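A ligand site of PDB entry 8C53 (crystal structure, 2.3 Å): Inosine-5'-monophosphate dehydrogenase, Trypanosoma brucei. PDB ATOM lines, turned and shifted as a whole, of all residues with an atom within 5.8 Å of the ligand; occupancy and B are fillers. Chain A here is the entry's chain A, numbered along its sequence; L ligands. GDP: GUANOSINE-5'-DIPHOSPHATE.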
ATOM      1  N   ARG A  98     -19.875 -27.760  22.222  1.00  0.00           N
ATOM      2  CA  ARG A  98     -19.340 -26.418  22.361  1.00  0.00           C
ATOM      3  C   ARG A  98     -18.973 -26.113  23.812  1.00  0.00           C
ATOM      4  O   ARG A  98     -17.926 -25.524  24.084  1.00  0.00           O
ATOM      5  CB  ARG A  98     -20.340 -25.373  21.838  1.00  0.00           C
ATOM      6  CG  ARG A  98     -19.836 -23.935  21.962  1.00  0.00           C
ATOM      7  CD  ARG A  98     -20.804 -22.907  21.353  1.00  0.00           C
ATOM      8  NE  ARG A  98     -21.779 -23.498  20.445  1.00  0.00           N
ATOM      9  CZ  ARG A  98     -21.483 -23.980  19.246  1.00  0.00           C
ATOM     10  NH1 ARG A  98     -20.253 -23.955  18.769  1.00  0.00           N
ATOM     11  NH2 ARG A  98     -22.453 -24.517  18.504  1.00  0.00           N
ATOM     12  N   ARG A 101     -15.758 -27.832  24.548  1.00  0.00           N
ATOM     13  CA  ARG A 101     -14.648 -27.084  23.966  1.00  0.00           C
ATOM     14  C   ARG A 101     -14.317 -25.852  24.797  1.00  0.00           C
ATOM     15  O   ARG A 101     -13.139 -25.541  25.010  1.00  0.00           O
ATOM     16  CB  ARG A 101     -14.991 -26.683  22.533  1.00  0.00           C
ATOM     17  CG  ARG A 101     -14.561 -27.698  21.479  1.00  0.00           C
ATOM     18  CD  ARG A 101     -14.859 -27.183  20.081  1.00  0.00           C
ATOM     19  NE  ARG A 101     -16.165 -27.640  19.600  1.00  0.00           N
ATOM     20  CZ  ARG A 101     -17.198 -26.847  19.366  1.00  0.00           C
ATOM     21  NH1 ARG A 101     -17.117 -25.540  19.539  1.00  0.00           N
ATOM     22  NH2 ARG A 101     -18.348 -27.389  18.961  1.00  0.00           N
ATOM     23  N   LEU A 105     -10.433 -25.615  26.089  1.00  0.00           N
ATOM     24  CA  LEU A 105      -9.561 -24.629  25.476  1.00  0.00           C
ATOM     25  C   LEU A 105      -9.404 -23.357  26.307  1.00  0.00           C
ATOM     26  O   LEU A 105      -8.781 -22.395  25.851  1.00  0.00           O
ATOM     27  CB  LEU A 105     -10.068 -24.279  24.092  1.00  0.00           C
ATOM     28  CG  LEU A 105     -10.426 -25.475  23.207  1.00  0.00           C
ATOM     29  CD1 LEU A 105     -11.056 -25.010  21.889  1.00  0.00           C
ATOM     30  CD2 LEU A 105      -9.190 -26.326  22.941  1.00  0.00           C
ATOM     31  N   TYR A 106      -9.985 -23.325  27.504  1.00  0.00           N
ATOM     32  CA  TYR A 106      -9.801 -22.170  28.378  1.00  0.00           C
ATOM     33  C   TYR A 106      -8.346 -22.045  28.824  1.00  0.00           C
ATOM     34  O   TYR A 106      -7.753 -20.966  28.748  1.00  0.00           O
ATOM     35  CB  TYR A 106     -10.714 -22.294  29.599  1.00  0.00           C
ATOM     36  CG  TYR A 106     -10.499 -21.238  30.654  1.00  0.00           C
ATOM     37  CD1 TYR A 106     -10.865 -19.911  30.425  1.00  0.00           C
ATOM     38  CD2 TYR A 106      -9.952 -21.574  31.881  1.00  0.00           C
ATOM     39  CE1 TYR A 106     -10.690 -18.950  31.394  1.00  0.00           C
ATOM     40  CE2 TYR A 106      -9.769 -20.619  32.864  1.00  0.00           C
ATOM     41  CZ  TYR A 106     -10.130 -19.304  32.614  1.00  0.00           C
ATOM     42  OH  TYR A 106      -9.939 -18.357  33.589  1.00  0.00           O
ATOM     43  N   ASN A 108      -4.389 -23.458  28.403  1.00  0.00           N
ATOM     44  CA  ASN A 108      -3.515 -24.114  27.450  1.00  0.00           C
ATOM     45  C   ASN A 108      -2.065 -23.846  27.810  1.00  0.00           C
ATOM     46  O   ASN A 108      -1.753 -22.989  28.654  1.00  0.00           O
ATOM     47  CB  ASN A 108      -3.737 -23.645  26.004  1.00  0.00           C
ATOM     48  CG  ASN A 108      -5.189 -23.396  25.693  1.00  0.00           C
ATOM     49  OD1 ASN A 108      -5.827 -22.521  26.295  1.00  0.00           O
ATOM     50  ND2 ASN A 108      -5.726 -24.130  24.723  1.00  0.00           N
ATOM     51  N   ILE A 111      -1.295 -22.487  22.551  1.00  0.00           N
ATOM     52  CA  ILE A 111      -2.643 -22.384  21.983  1.00  0.00           C
ATOM     53  C   ILE A 111      -2.552 -22.684  20.496  1.00  0.00           C
ATOM     54  O   ILE A 111      -1.910 -21.946  19.743  1.00  0.00           O
ATOM     55  CB  ILE A 111      -3.240 -20.993  22.231  1.00  0.00           C
ATOM     56  CG1 ILE A 111      -3.391 -20.732  23.730  1.00  0.00           C
ATOM     57  CG2 ILE A 111      -4.576 -20.876  21.536  1.00  0.00           C
ATOM     58  CD1 ILE A 111      -3.609 -19.282  24.078  1.00  0.00           C
ATOM     59  N   MET A 112      -3.192 -23.765  20.059  1.00  0.00           N
ATOM     60  CA  MET A 112      -2.931 -24.300  18.725  1.00  0.00           C
ATOM     61  C   MET A 112      -3.800 -23.691  17.633  1.00  0.00           C
ATOM     62  O   MET A 112      -3.377 -23.650  16.469  1.00  0.00           O
ATOM     63  CB  MET A 112      -3.113 -25.826  18.723  1.00  0.00           C
ATOM     64  CG  MET A 112      -2.235 -26.530  19.730  1.00  0.00           C
ATOM     65  SD  MET A 112      -0.482 -26.180  19.520  1.00  0.00           S
ATOM     66  CE  MET A 112      -0.302 -26.292  17.730  1.00  0.00           C
ATOM     67  N   LYS A 113      -4.995 -23.226  17.952  1.00  0.00           N
ATOM     68  CA  LYS A 113      -5.888 -22.615  16.971  1.00  0.00           C
ATOM     69  C   LYS A 113      -6.267 -21.236  17.478  1.00  0.00           C
ATOM     70  O   LYS A 113      -7.432 -20.978  17.809  1.00  0.00           O
ATOM     71  CB  LYS A 113      -7.115 -23.478  16.724  1.00  0.00           C
ATOM     72  CG  LYS A 113      -6.937 -24.497  15.605  1.00  0.00           C
ATOM     73  CD  LYS A 113      -7.897 -25.657  15.742  1.00  0.00           C
ATOM     74  CE  LYS A 113      -8.494 -26.038  14.394  1.00  0.00           C
ATOM     75  NZ  LYS A 113      -9.298 -27.308  14.469  1.00  0.00           N
ATOM     76  N   PRO A 114      -5.298 -20.315  17.563  1.00  0.00           N
ATOM     77  CA  PRO A 114      -5.577 -19.010  18.166  1.00  0.00           C
ATOM     78  C   PRO A 114      -6.690 -18.304  17.403  1.00  0.00           C
ATOM     79  O   PRO A 114      -6.714 -18.284  16.178  1.00  0.00           O
ATOM     80  CB  PRO A 114      -4.246 -18.263  18.036  1.00  0.00           C
ATOM     81  CG  PRO A 114      -3.202 -19.343  17.749  1.00  0.00           C
ATOM     82  CD  PRO A 114      -3.948 -20.381  16.954  1.00  0.00           C
ATOM     83  N   LYS A 115      -7.622 -17.732  18.151  1.00  0.00           N
ATOM     84  CA  LYS A 115      -8.657 -16.915  17.528  1.00  0.00           C
ATOM     85  C   LYS A 115      -7.975 -15.807  16.728  1.00  0.00           C
ATOM     86  O   LYS A 115      -7.141 -15.068  17.262  1.00  0.00           O
ATOM     87  CB  LYS A 115      -9.566 -16.308  18.593  1.00  0.00           C
ATOM     88  CG  LYS A 115     -10.830 -15.685  18.027  1.00  0.00           C
ATOM     89  CD  LYS A 115     -12.037 -16.587  18.243  1.00  0.00           C
ATOM     90  CE  LYS A 115     -13.185 -16.227  17.310  1.00  0.00           C
ATOM     91  NZ  LYS A 115     -12.917 -16.666  15.913  1.00  0.00           N
ATOM     92  N   SER A 116      -8.322 -15.715  15.445  1.00  0.00           N
ATOM     93  CA  SER A 116      -7.675 -14.756  14.554  1.00  0.00           C
ATOM     94  C   SER A 116      -8.703 -14.162  13.607  1.00  0.00           C
ATOM     95  O   SER A 116      -9.710 -14.793  13.282  1.00  0.00           O
ATOM     96  CB  SER A 116      -6.524 -15.414  13.790  1.00  0.00           C
ATOM     97  OG  SER A 116      -7.000 -16.052  12.614  1.00  0.00           O
ATOM     98  N   LYS A 133     -16.866 -14.654  24.512  1.00  0.00           N
ATOM     99  CA  LYS A 133     -15.984 -15.782  24.801  1.00  0.00           C
ATOM    100  C   LYS A 133     -14.882 -15.432  25.785  1.00  0.00           C
ATOM    101  O   LYS A 133     -14.204 -16.335  26.270  1.00  0.00           O
ATOM    102  CB  LYS A 133     -15.370 -16.310  23.504  1.00  0.00           C
ATOM    103  CG  LYS A 133     -16.391 -16.513  22.386  1.00  0.00           C
ATOM    104  CD  LYS A 133     -16.158 -17.812  21.629  1.00  0.00           C
ATOM    105  CE  LYS A 133     -16.970 -17.865  20.350  1.00  0.00           C
ATOM    106  NZ  LYS A 133     -16.583 -19.022  19.494  1.00  0.00           N
ATOM    107  N   ILE A 135     -11.929 -13.838  25.564  1.00  0.00           N
ATOM    108  CA  ILE A 135     -10.537 -13.972  25.157  1.00  0.00           C
ATOM    109  C   ILE A 135     -10.093 -12.686  24.475  1.00  0.00           C
ATOM    110  O   ILE A 135     -10.795 -12.149  23.611  1.00  0.00           O
ATOM    111  CB  ILE A 135     -10.330 -15.191  24.229  1.00  0.00           C
ATOM    112  CG1 ILE A 135     -10.969 -14.947  22.869  1.00  0.00           C
ATOM    113  CG2 ILE A 135     -10.890 -16.445  24.903  1.00  0.00           C
ATOM    114  CD1 ILE A 135     -11.090 -16.195  21.992  1.00  0.00           C
ATOM    115  N   SER A 136      -8.925 -12.180  24.885  1.00  0.00           N
ATOM    116  CA  SER A 136      -8.266 -11.039  24.278  1.00  0.00           C
ATOM    117  C   SER A 136      -7.081 -11.531  23.449  1.00  0.00           C
ATOM    118  O   SER A 136      -6.918 -12.731  23.183  1.00  0.00           O
ATOM    119  CB  SER A 136      -7.830 -10.041  25.355  1.00  0.00           C
ATOM    120  OG  SER A 136      -7.415  -8.802  24.776  1.00  0.00           O
ATOM    121  N   GLY A 137      -6.233 -10.604  23.008  1.00  0.00           N
ATOM    122  CA  GLY A 137      -5.050 -10.966  22.261  1.00  0.00           C
ATOM    123  C   GLY A 137      -5.387 -11.610  20.929  1.00  0.00           C
ATOM    124  O   GLY A 137      -4.833 -12.644  20.569  1.00  0.00           O
ATOM    125  N   ILE A 138      -6.319 -11.001  20.208  1.00  0.00           N
ATOM    126  CA  ILE A 138      -6.787 -11.567  18.944  1.00  0.00           C
ATOM    127  C   ILE A 138      -5.743 -11.319  17.869  1.00  0.00           C
ATOM    128  O   ILE A 138      -5.251 -10.197  17.704  1.00  0.00           O
ATOM    129  CB  ILE A 138      -8.141 -10.969  18.544  1.00  0.00           C
ATOM    130  CG1 ILE A 138      -9.163 -11.076  19.692  1.00  0.00           C
ATOM    131  CG2 ILE A 138      -8.664 -11.627  17.288  1.00  0.00           C
ATOM    132  CD1 ILE A 138      -8.979 -12.291  20.606  1.00  0.00           C
ATOM    133  N   LEU A 139      -5.378 -12.373  17.137  1.00  0.00           N
ATOM    134  CA  LEU A 139      -4.392 -12.250  16.085  1.00  0.00           C
ATOM    135  C   LEU A 139      -5.053 -11.762  14.800  1.00  0.00           C
ATOM    136  O   LEU A 139      -6.128 -12.220  14.429  1.00  0.00           O
ATOM    137  CB  LEU A 139      -3.691 -13.579  15.839  1.00  0.00           C
ATOM    138  CG  LEU A 139      -3.018 -14.250  17.030  1.00  0.00           C
ATOM    139  CD1 LEU A 139      -2.132 -15.403  16.571  1.00  0.00           C
ATOM    140  CD2 LEU A 139      -2.207 -13.258  17.840  1.00  0.00           C
ATOM    141  N   TYR A 202       1.081 -11.690  25.265  1.00  0.00           N
ATOM    142  CA  TYR A 202       0.987 -12.789  24.307  1.00  0.00           C
ATOM    143  C   TYR A 202       2.287 -12.929  23.542  1.00  0.00           C
ATOM    144  O   TYR A 202       3.053 -11.976  23.388  1.00  0.00           O
ATOM    145  CB  TYR A 202      -0.194 -12.559  23.354  1.00  0.00           C
ATOM    146  CG  TYR A 202      -1.522 -12.539  24.058  1.00  0.00           C
ATOM    147  CD1 TYR A 202      -2.242 -13.711  24.252  1.00  0.00           C
ATOM    148  CD2 TYR A 202      -2.055 -11.357  24.557  1.00  0.00           C
ATOM    149  CE1 TYR A 202      -3.454 -13.706  24.920  1.00  0.00           C
ATOM    150  CE2 TYR A 202      -3.263 -11.339  25.229  1.00  0.00           C
ATOM    151  CZ  TYR A 202      -3.954 -12.521  25.402  1.00  0.00           C
ATOM    152  OH  TYR A 202      -5.169 -12.510  26.047  1.00  0.00           O
ATOM    153  N   LEU A 215       0.325 -20.023  19.864  1.00  0.00           N
ATOM    154  CA  LEU A 215       0.289 -18.803  20.662  1.00  0.00           C
ATOM    155  C   LEU A 215       0.408 -19.129  22.131  1.00  0.00           C
ATOM    156  O   LEU A 215      -0.233 -20.063  22.615  1.00  0.00           O
ATOM    157  CB  LEU A 215      -1.020 -18.046  20.392  1.00  0.00           C
ATOM    158  CG  LEU A 215      -1.286 -16.780  21.197  1.00  0.00           C
ATOM    159  CD1 LEU A 215      -0.273 -15.718  20.851  1.00  0.00           C
ATOM    160  CD2 LEU A 215      -2.702 -16.286  20.922  1.00  0.00           C
ATOM    161  N   SER A 217      -0.062 -17.451  26.023  1.00  0.00           N
ATOM    162  CA  SER A 217      -0.801 -16.413  26.719  1.00  0.00           C
ATOM    163  C   SER A 217      -0.300 -16.304  28.144  1.00  0.00           C
ATOM    164  O   SER A 217      -0.206 -17.306  28.850  1.00  0.00           O
ATOM    165  CB  SER A 217      -2.296 -16.729  26.722  1.00  0.00           C
ATOM    166  OG  SER A 217      -2.969 -16.015  27.733  1.00  0.00           O
ATOM    167  N   ARG A 219      -1.915 -15.102  30.491  1.00  0.00           N
ATOM    168  CA  ARG A 219      -3.020 -15.458  31.368  1.00  0.00           C
ATOM    169  C   ARG A 219      -2.950 -16.917  31.785  1.00  0.00           C
ATOM    170  O   ARG A 219      -3.335 -17.257  32.899  1.00  0.00           O
ATOM    171  CB  ARG A 219      -4.354 -15.161  30.674  1.00  0.00           C
ATOM    172  CG  ARG A 219      -4.659 -13.677  30.594  1.00  0.00           C
ATOM    173  CD  ARG A 219      -5.976 -13.382  29.918  1.00  0.00           C
ATOM    174  NE  ARG A 219      -6.291 -11.954  29.982  1.00  0.00           N
ATOM    175  CZ  ARG A 219      -5.661 -11.013  29.304  1.00  0.00           C
ATOM    176  NH1 ARG A 219      -4.658 -11.302  28.491  1.00  0.00           N
ATOM    177  NH2 ARG A 219      -6.044  -9.743  29.440  1.00  0.00           N
HETATM  178  PB  GDP L   1     -16.037 -21.912  17.613  1.00  0.00           P
HETATM  179  O1B GDP L   1     -16.069 -23.178  16.799  1.00  0.00           O
HETATM  180  O2B GDP L   1     -17.265 -21.866  18.524  1.00  0.00           O
HETATM  181  O3B GDP L   1     -16.024 -20.716  16.681  1.00  0.00           O
HETATM  182  O3A GDP L   1     -14.646 -21.899  18.540  1.00  0.00           O
HETATM  183  PA  GDP L   1     -13.685 -20.543  18.763  1.00  0.00           P
HETATM  184  O1A GDP L   1     -13.684 -19.738  17.476  1.00  0.00           O
HETATM  185  O2A GDP L   1     -14.246 -19.707  19.887  1.00  0.00           O
HETATM  186  O5' GDP L   1     -12.142 -21.010  19.124  1.00  0.00           O
HETATM  187  C5' GDP L   1     -11.408 -20.295  20.076  1.00  0.00           C
HETATM  188  C4' GDP L   1      -9.972 -20.598  19.870  1.00  0.00           C
HETATM  189  O4' GDP L   1      -9.041 -19.461  20.666  1.00  0.00           O
HETATM  190  C3' GDP L   1      -9.675 -21.761  20.364  1.00  0.00           C
HETATM  191  O3' GDP L   1      -8.890 -22.512  19.346  1.00  0.00           O
HETATM  192  C2' GDP L   1      -8.790 -21.507  21.635  1.00  0.00           C
HETATM  193  O2' GDP L   1      -7.885 -22.449  21.789  1.00  0.00           O
HETATM  194  C1' GDP L   1      -8.112 -20.127  21.289  1.00  0.00           C
HETATM  195  N9  GDP L   1      -7.713 -19.340  22.434  1.00  0.00           N
HETATM  196  C8  GDP L   1      -7.714 -19.680  23.698  1.00  0.00           C
HETATM  197  N7  GDP L   1      -7.256 -18.666  24.419  1.00  0.00           N
HETATM  198  C5  GDP L   1      -6.938 -17.657  23.599  1.00  0.00           C
HETATM  199  C6  GDP L   1      -6.386 -16.276  23.806  1.00  0.00           C
HETATM  200  O6  GDP L   1      -6.145 -15.905  24.893  1.00  0.00           O
HETATM  201  N1  GDP L   1      -6.150 -15.429  22.671  1.00  0.00           N
HETATM  202  C2  GDP L   1      -6.455 -15.902  21.341  1.00  0.00           C
HETATM  203  N2  GDP L   1      -6.230 -15.053  20.178  1.00  0.00           N
HETATM  204  N3  GDP L   1      -6.997 -17.231  21.156  1.00  0.00           N
HETATM  205  C4  GDP L   1      -7.230 -18.104  22.334  1.00  0.00           C
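O of Ser 136 sits at hydrogen-bond distance from N1 of the ligand (2.9 Å).
The backbone carbonyl oxygen (O) of Gly 137 lies within hydrogen-bond range of a nitrogen (N2) of the ligand, 2.8 Å away.
The backbone carbonyl oxygen of Lys 115 is in hydrogen-bond range of a nitrogen (N2) of the ligand, 3.1 Å away.
An oxygen (O1A) of the ligand lies within salt-bridge range of the side-chain amino group (NZ) of Lys 115, 3.5 Å away.
NZ of Lys 133 is in salt-bridge range of O2A of the ligand (2.5 Å).
NH1 of Arg 101 lies within salt-bridge range of O1B of the ligand.
O2B of the ligand is in salt-bridge range of NH1 of Arg 98, at 3.7 Å.
O3' of the ligand is in hydrogen-bond range of O of Lys 113, 2.6 Å away.
The backbone NH (N) of Lys 115 sits at hydrogen-bond distance from a nitrogen (N3) of the ligand, 3.1 Å away.
The backbone carbonyl oxygen (O) of Lys 115 is in hydrogen-bond range of the backbone NH (N) of Leu 139 (3.2 Å).
The guanidinium group of Arg 219 sits at hydrogen-bond distance from the side-chain hydroxyl of Tyr 202, at 2.8 Å.
The backbone carbonyl oxygen (O) of Leu 105 sits close to the side-chain amide oxygen (OD1) of Asn 108 (3.0 Å).
O of Ser 136 is in hydrogen-bond range of OH of Tyr 202, 3.4 Å away.
The backbone NH (N) of Ile 111 is in hydrogen-bond range of the backbone carbonyl oxygen (O) of Leu 215 (2.6 Å).
Merely in contact with the ligand: Tyr 202, Ile 111, Leu 105, Ile 138, Pro 114 and Leu 215.
Hydrophobic or aromatic side chains within 4 Å of the ligand: Leu 105, Ile 111, Ile 138, Tyr 202 and Leu 215.
The nearest printed residue that does not touch the ligand is Asn 108 (4.01 Å).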
